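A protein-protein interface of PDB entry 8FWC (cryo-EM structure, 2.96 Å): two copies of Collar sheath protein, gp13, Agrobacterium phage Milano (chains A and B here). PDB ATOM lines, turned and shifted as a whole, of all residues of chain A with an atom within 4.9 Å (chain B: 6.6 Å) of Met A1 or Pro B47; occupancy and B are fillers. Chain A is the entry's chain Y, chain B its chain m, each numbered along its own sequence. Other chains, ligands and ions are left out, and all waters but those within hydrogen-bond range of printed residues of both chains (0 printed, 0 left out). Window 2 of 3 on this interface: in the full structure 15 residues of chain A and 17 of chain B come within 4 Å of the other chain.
Among the printed residues, pairs that only touch across the chains: Tyr A2 with Asn B10, Asn A35 with Arg B9, Asn A35 with Phe B216, Tyr A2 with Gly B11, Met A1 with Leu B48, Asn A35 with Trp B44, Met A1 with Asn B10, Tyr A2 with Arg B9 and Gly A36 with Phe B216.
Printed residues of chain B within 4 Å of Met A1: Pro B8 (3.4 Å), Arg B9 (3.3 Å), Asn B10 (3.8 Å), Pro B47 (3.8 Å) and Leu B48 (3.6 Å). Pro B47 touches one residue of chain A. Printed residues of chain A within 4 Å of Arg B9: Met A1, Tyr A2 and Asn A35. Printed residues of chain B within 4 Å of Tyr A2: Arg B9 (3.9 Å), Asn B10 (3.2 Å) and Gly B11 (3.5 Å). Printed residues of chain A within 4 Å of Phe B216: Asn A35 (3.5 Å) and Gly A36 (3.9 Å). Printed residues of chain B within 4 Å of Asn A35: Arg B9, Trp B44 and Phe B216. Of the printed residues of chain A, Leu B48 touches Met A1 (3.6 Å). Ala B46 touches none of the printed residues of chain A. The nearest residue of chain B that does not touch Met A1 is Trp B44 (4.4 Å). The nearest printed residue of chain A that does not touch Arg B9 is Gly A36 (5.8 Å).
The backbone carbonyl oxygen of Pro B8 lies close to the side-chain amide oxygen of Asn B10, at 3.1 Å. O of Tyr A2 is in hydrogen-bond range of N of Met A38 (2.8 Å). O of Gly A36 lies within hydrogen-bond range of N of Tyr A2, at 3.0 Å.
Among the printed residues, no Asp or Glu carboxylate lies within 4 Å of a Lys or Arg side-chain nitrogen of the other chain.
The backbone NH (N) of Met A1 is in hydrogen-bond range of the backbone carbonyl oxygen (O) of Arg B9, at 3.3 Å. N of Met A1 sits at hydrogen-bond distance from O of Pro B8, 3.4 Å away. The backbone carbonyl oxygen (O) of Pro B47 lies close to the side-chain sulfur (SD) of Met A1 (3.8 Å).
No position is printed for both chains. Of the 12 pairs that touch across the chains among the printed residues, none has its exchanged pair printed and touching as well.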
ATOM      1  N   MET A   1      11.875  -3.599  23.885  1.00  0.00           N
ATOM      2  CA  MET A   1      11.721  -3.870  22.465  1.00  0.00           C
ATOM      3  C   MET A   1      10.341  -4.434  22.164  1.00  0.00           C
ATOM      4  O   MET A   1       9.938  -5.439  22.734  1.00  0.00           O
ATOM      5  CB  MET A   1      12.806  -4.834  21.992  1.00  0.00           C
ATOM      6  CG  MET A   1      12.456  -5.613  20.750  1.00  0.00           C
ATOM      7  SD  MET A   1      13.837  -6.568  20.125  1.00  0.00           S
ATOM      8  CE  MET A   1      14.565  -5.386  19.000  1.00  0.00           C
ATOM      9  N   TYR A   2       9.615  -3.769  21.275  1.00  0.00           N
ATOM     10  CA  TYR A   2       8.309  -4.230  20.836  1.00  0.00           C
ATOM     11  C   TYR A   2       8.466  -5.316  19.788  1.00  0.00           C
ATOM     12  O   TYR A   2       9.366  -5.268  18.951  1.00  0.00           O
ATOM     13  CB  TYR A   2       7.500  -3.075  20.255  1.00  0.00           C
ATOM     14  CG  TYR A   2       6.749  -2.280  21.282  1.00  0.00           C
ATOM     15  CD1 TYR A   2       5.538  -2.723  21.769  1.00  0.00           C
ATOM     16  CD2 TYR A   2       7.255  -1.092  21.769  1.00  0.00           C
ATOM     17  CE1 TYR A   2       4.849  -2.007  22.704  1.00  0.00           C
ATOM     18  CE2 TYR A   2       6.572  -0.370  22.708  1.00  0.00           C
ATOM     19  CZ  TYR A   2       5.369  -0.832  23.171  1.00  0.00           C
ATOM     20  OH  TYR A   2       4.676  -0.115  24.113  1.00  0.00           O
ATOM     21  N   PHE A   3       7.574  -6.295  19.827  1.00  0.00           N
ATOM     22  CA  PHE A   3       7.588  -7.357  18.832  1.00  0.00           C
ATOM     23  C   PHE A   3       6.171  -7.587  18.348  1.00  0.00           C
ATOM     24  O   PHE A   3       5.304  -7.976  19.133  1.00  0.00           O
ATOM     25  CB  PHE A   3       8.173  -8.648  19.398  1.00  0.00           C
ATOM     26  CG  PHE A   3       8.177  -9.778  18.422  1.00  0.00           C
ATOM     27  CD1 PHE A   3       9.213  -9.921  17.523  1.00  0.00           C
ATOM     28  CD2 PHE A   3       7.143 -10.689  18.390  1.00  0.00           C
ATOM     29  CE1 PHE A   3       9.220 -10.949  16.619  1.00  0.00           C
ATOM     30  CE2 PHE A   3       7.145 -11.722  17.484  1.00  0.00           C
ATOM     31  CZ  PHE A   3       8.186 -11.851  16.599  1.00  0.00           C
ATOM     32  N   ASN A  35      13.334   3.677  21.479  1.00  0.00           N
ATOM     33  CA  ASN A  35      13.095   2.258  21.666  1.00  0.00           C
ATOM     34  C   ASN A  35      13.362   1.508  20.361  1.00  0.00           C
ATOM     35  O   ASN A  35      13.788   2.099  19.367  1.00  0.00           O
ATOM     36  CB  ASN A  35      11.669   2.065  22.180  1.00  0.00           C
ATOM     37  CG  ASN A  35      11.483   0.752  22.881  1.00  0.00           C
ATOM     38  OD1 ASN A  35      12.405  -0.052  22.961  1.00  0.00           O
ATOM     39  ND2 ASN A  35      10.287   0.519  23.392  1.00  0.00           N
ATOM     40  N   GLY A  36      13.106   0.205  20.351  1.00  0.00           N
ATOM     41  CA  GLY A  36      13.288  -0.586  19.153  1.00  0.00           C
ATOM     42  C   GLY A  36      12.098  -1.474  18.873  1.00  0.00           C
ATOM     43  O   GLY A  36      11.527  -2.051  19.798  1.00  0.00           O
ATOM     44  N   MET A  38      10.338  -4.608  16.421  1.00  0.00           N
ATOM     45  CA  MET A  38      10.553  -5.735  15.529  1.00  0.00           C
ATOM     46  C   MET A  38       9.216  -6.237  15.009  1.00  0.00           C
ATOM     47  O   MET A  38       8.283  -6.451  15.785  1.00  0.00           O
ATOM     48  CB  MET A  38      11.285  -6.867  16.239  1.00  0.00           C
ATOM     49  CG  MET A  38      12.790  -6.772  16.161  1.00  0.00           C
ATOM     50  SD  MET A  38      13.609  -8.112  17.032  1.00  0.00           S
ATOM     51  CE  MET A  38      12.559  -9.483  16.584  1.00  0.00           C
ATOM     52  N   PRO B   8      10.396  -3.504  30.771  1.00  0.00           N
ATOM     53  CA  PRO B   8      11.108  -3.831  29.533  1.00  0.00           C
ATOM     54  C   PRO B   8      10.548  -3.197  28.268  1.00  0.00           C
ATOM     55  O   PRO B   8      11.078  -3.476  27.190  1.00  0.00           O
ATOM     56  CB  PRO B   8      11.014  -5.355  29.486  1.00  0.00           C
ATOM     57  CG  PRO B   8       9.765  -5.667  30.182  1.00  0.00           C
ATOM     58  CD  PRO B   8       9.550  -4.617  31.223  1.00  0.00           C
ATOM     59  N   ARG B   9       9.528  -2.346  28.349  1.00  0.00           N
ATOM     60  CA  ARG B   9       8.972  -1.649  27.187  1.00  0.00           C
ATOM     61  C   ARG B   9       8.506  -2.630  26.112  1.00  0.00           C
ATOM     62  O   ARG B   9       8.919  -2.566  24.955  1.00  0.00           O
ATOM     63  CB  ARG B   9       9.976  -0.658  26.611  1.00  0.00           C
ATOM     64  CG  ARG B   9      10.752   0.122  27.647  1.00  0.00           C
ATOM     65  CD  ARG B   9       9.849   0.928  28.530  1.00  0.00           C
ATOM     66  NE  ARG B   9       8.997   1.825  27.768  1.00  0.00           N
ATOM     67  CZ  ARG B   9       7.879   2.344  28.251  1.00  0.00           C
ATOM     68  NH1 ARG B   9       7.502   2.036  29.479  1.00  0.00           N
ATOM     69  NH2 ARG B   9       7.138   3.157  27.516  1.00  0.00           N
ATOM     70  N   ASN B  10       7.631  -3.554  26.509  1.00  0.00           N
ATOM     71  CA  ASN B  10       7.002  -4.510  25.606  1.00  0.00           C
ATOM     72  C   ASN B  10       5.563  -4.174  25.275  1.00  0.00           C
ATOM     73  O   ASN B  10       5.000  -4.782  24.363  1.00  0.00           O
ATOM     74  CB  ASN B  10       7.008  -5.912  26.209  1.00  0.00           C
ATOM     75  CG  ASN B  10       8.380  -6.439  26.427  1.00  0.00           C
ATOM     76  OD1 ASN B  10       9.132  -5.917  27.228  1.00  0.00           O
ATOM     77  ND2 ASN B  10       8.725  -7.493  25.709  1.00  0.00           N
ATOM     78  N   GLY B  11       4.945  -3.260  26.012  1.00  0.00           N
ATOM     79  CA  GLY B  11       3.502  -3.184  26.024  1.00  0.00           C
ATOM     80  C   GLY B  11       2.883  -4.116  27.037  1.00  0.00           C
ATOM     81  O   GLY B  11       1.699  -4.444  26.928  1.00  0.00           O
ATOM     82  N   TYR B  41      19.173  -3.697  33.779  1.00  0.00           N
ATOM     83  CA  TYR B  41      18.565  -3.399  32.492  1.00  0.00           C
ATOM     84  C   TYR B  41      18.428  -4.615  31.595  1.00  0.00           C
ATOM     85  O   TYR B  41      18.167  -4.449  30.402  1.00  0.00           O
ATOM     86  CB  TYR B  41      19.380  -2.336  31.768  1.00  0.00           C
ATOM     87  CG  TYR B  41      19.157  -0.955  32.299  1.00  0.00           C
ATOM     88  CD1 TYR B  41      19.800  -0.518  33.435  1.00  0.00           C
ATOM     89  CD2 TYR B  41      18.297  -0.087  31.666  1.00  0.00           C
ATOM     90  CE1 TYR B  41      19.593   0.743  33.922  1.00  0.00           C
ATOM     91  CE2 TYR B  41      18.086   1.172  32.145  1.00  0.00           C
ATOM     92  CZ  TYR B  41      18.733   1.583  33.271  1.00  0.00           C
ATOM     93  OH  TYR B  41      18.513   2.849  33.746  1.00  0.00           O
ATOM     94  N   ALA B  42      18.611  -5.824  32.124  1.00  0.00           N
ATOM     95  CA  ALA B  42      18.614  -7.012  31.280  1.00  0.00           C
ATOM     96  C   ALA B  42      17.300  -7.183  30.537  1.00  0.00           C
ATOM     97  O   ALA B  42      17.290  -7.577  29.369  1.00  0.00           O
ATOM     98  CB  ALA B  42      18.910  -8.251  32.121  1.00  0.00           C
ATOM     99  N   ALA B  43      16.179  -6.896  31.191  1.00  0.00           N
ATOM    100  CA  ALA B  43      14.888  -7.124  30.555  1.00  0.00           C
ATOM    101  C   ALA B  43      14.665  -6.233  29.343  1.00  0.00           C
ATOM    102  O   ALA B  43      13.887  -6.598  28.461  1.00  0.00           O
ATOM    103  CB  ALA B  43      13.762  -6.913  31.565  1.00  0.00           C
ATOM    104  N   TRP B  44      15.329  -5.085  29.274  1.00  0.00           N
ATOM    105  CA  TRP B  44      15.131  -4.136  28.187  1.00  0.00           C
ATOM    106  C   TRP B  44      16.225  -4.202  27.139  1.00  0.00           C
ATOM    107  O   TRP B  44      15.933  -4.124  25.944  1.00  0.00           O
ATOM    108  CB  TRP B  44      15.054  -2.712  28.741  1.00  0.00           C
ATOM    109  CG  TRP B  44      15.097  -1.629  27.710  1.00  0.00           C
ATOM    110  CD1 TRP B  44      14.099  -1.263  26.868  1.00  0.00           C
ATOM    111  CD2 TRP B  44      16.191  -0.754  27.435  1.00  0.00           C
ATOM    112  NE1 TRP B  44      14.502  -0.222  26.077  1.00  0.00           N
ATOM    113  CE2 TRP B  44      15.788   0.108  26.408  1.00  0.00           C
ATOM    114  CE3 TRP B  44      17.477  -0.622  27.955  1.00  0.00           C
ATOM    115  CZ2 TRP B  44      16.619   1.083  25.893  1.00  0.00           C
ATOM    116  CZ3 TRP B  44      18.296   0.347  27.443  1.00  0.00           C
ATOM    117  CH2 TRP B  44      17.868   1.186  26.425  1.00  0.00           C
ATOM    118  N   SER B  45      17.473  -4.351  27.556  1.00  0.00           N
ATOM    119  CA  SER B  45      18.603  -4.241  26.651  1.00  0.00           C
ATOM    120  C   SER B  45      19.081  -5.578  26.113  1.00  0.00           C
ATOM    121  O   SER B  45      19.945  -5.594  25.234  1.00  0.00           O
ATOM    122  CB  SER B  45      19.765  -3.550  27.354  1.00  0.00           C
ATOM    123  OG  SER B  45      20.974  -4.185  27.008  1.00  0.00           O
ATOM    124  N   ALA B  46      18.563  -6.699  26.616  1.00  0.00           N
ATOM    125  CA  ALA B  46      18.993  -7.988  26.084  1.00  0.00           C
ATOM    126  C   ALA B  46      18.351  -8.283  24.734  1.00  0.00           C
ATOM    127  O   ALA B  46      19.068  -8.677  23.802  1.00  0.00           O
ATOM    128  CB  ALA B  46      18.740  -9.096  27.105  1.00  0.00           C
ATOM    129  N   PRO B  47      17.033  -8.138  24.559  1.00  0.00           N
ATOM    130  CA  PRO B  47      16.469  -8.318  23.215  1.00  0.00           C
ATOM    131  C   PRO B  47      17.101  -7.430  22.165  1.00  0.00           C
ATOM    132  O   PRO B  47      17.267  -7.860  21.020  1.00  0.00           O
ATOM    133  CB  PRO B  47      14.991  -7.983  23.425  1.00  0.00           C
ATOM    134  CG  PRO B  47      14.739  -8.377  24.805  1.00  0.00           C
ATOM    135  CD  PRO B  47      15.962  -7.975  25.554  1.00  0.00           C
ATOM    136  N   LEU B  48      17.474  -6.207  22.515  1.00  0.00           N
ATOM    137  CA  LEU B  48      18.209  -5.347  21.593  1.00  0.00           C
ATOM    138  C   LEU B  48      19.629  -5.877  21.429  1.00  0.00           C
ATOM    139  O   LEU B  48      20.593  -5.298  21.922  1.00  0.00           O
ATOM    140  CB  LEU B  48      18.229  -3.915  22.106  1.00  0.00           C
ATOM    141  CG  LEU B  48      16.915  -3.216  22.403  1.00  0.00           C
ATOM    142  CD1 LEU B  48      17.206  -1.900  23.058  1.00  0.00           C
ATOM    143  CD2 LEU B  48      16.153  -3.001  21.133  1.00  0.00           C
ATOM    144  N   ARG B  49      19.744  -7.010  20.738  1.00  0.00           N
ATOM    145  CA  ARG B  49      21.031  -7.684  20.669  1.00  0.00           C
ATOM    146  C   ARG B  49      22.074  -6.749  20.082  1.00  0.00           C
ATOM    147  O   ARG B  49      22.036  -6.431  18.892  1.00  0.00           O
ATOM    148  CB  ARG B  49      20.939  -8.962  19.839  1.00  0.00           C
ATOM    149  CG  ARG B  49      19.880  -9.943  20.291  1.00  0.00           C
ATOM    150  CD  ARG B  49      19.915 -11.175  19.414  1.00  0.00           C
ATOM    151  NE  ARG B  49      20.367 -10.848  18.063  1.00  0.00           N
ATOM    152  CZ  ARG B  49      20.828 -11.736  17.187  1.00  0.00           C
ATOM    153  NH1 ARG B  49      20.907 -13.017  17.516  1.00  0.00           N
ATOM    154  NH2 ARG B  49      21.219 -11.340  15.983  1.00  0.00           N
ATOM    155  N   GLY B  50      23.003  -6.305  20.917  1.00  0.00           N
ATOM    156  CA  GLY B  50      23.994  -5.337  20.508  1.00  0.00           C
ATOM    157  C   GLY B  50      25.195  -5.368  21.421  1.00  0.00           C
ATOM    158  O   GLY B  50      25.638  -6.443  21.830  1.00  0.00           O
ATOM    159  N   PHE B 216      20.090   3.748  22.068  1.00  0.00           N
ATOM    160  CA  PHE B 216      18.764   3.420  22.574  1.00  0.00           C
ATOM    161  C   PHE B 216      18.656   3.994  23.973  1.00  0.00           C
ATOM    162  O   PHE B 216      19.353   3.535  24.878  1.00  0.00           O
ATOM    163  CB  PHE B 216      18.539   1.910  22.618  1.00  0.00           C
ATOM    164  CG  PHE B 216      18.358   1.272  21.283  1.00  0.00           C
ATOM    165  CD1 PHE B 216      17.149   1.335  20.637  1.00  0.00           C
ATOM    166  CD2 PHE B 216      19.380   0.567  20.695  1.00  0.00           C
ATOM    167  CE1 PHE B 216      16.974   0.732  19.423  1.00  0.00           C
ATOM    168  CE2 PHE B 216      19.206  -0.035  19.481  1.00  0.00           C
ATOM    169  CZ  PHE B 216      18.002   0.048  18.845  1.00  0.00           C
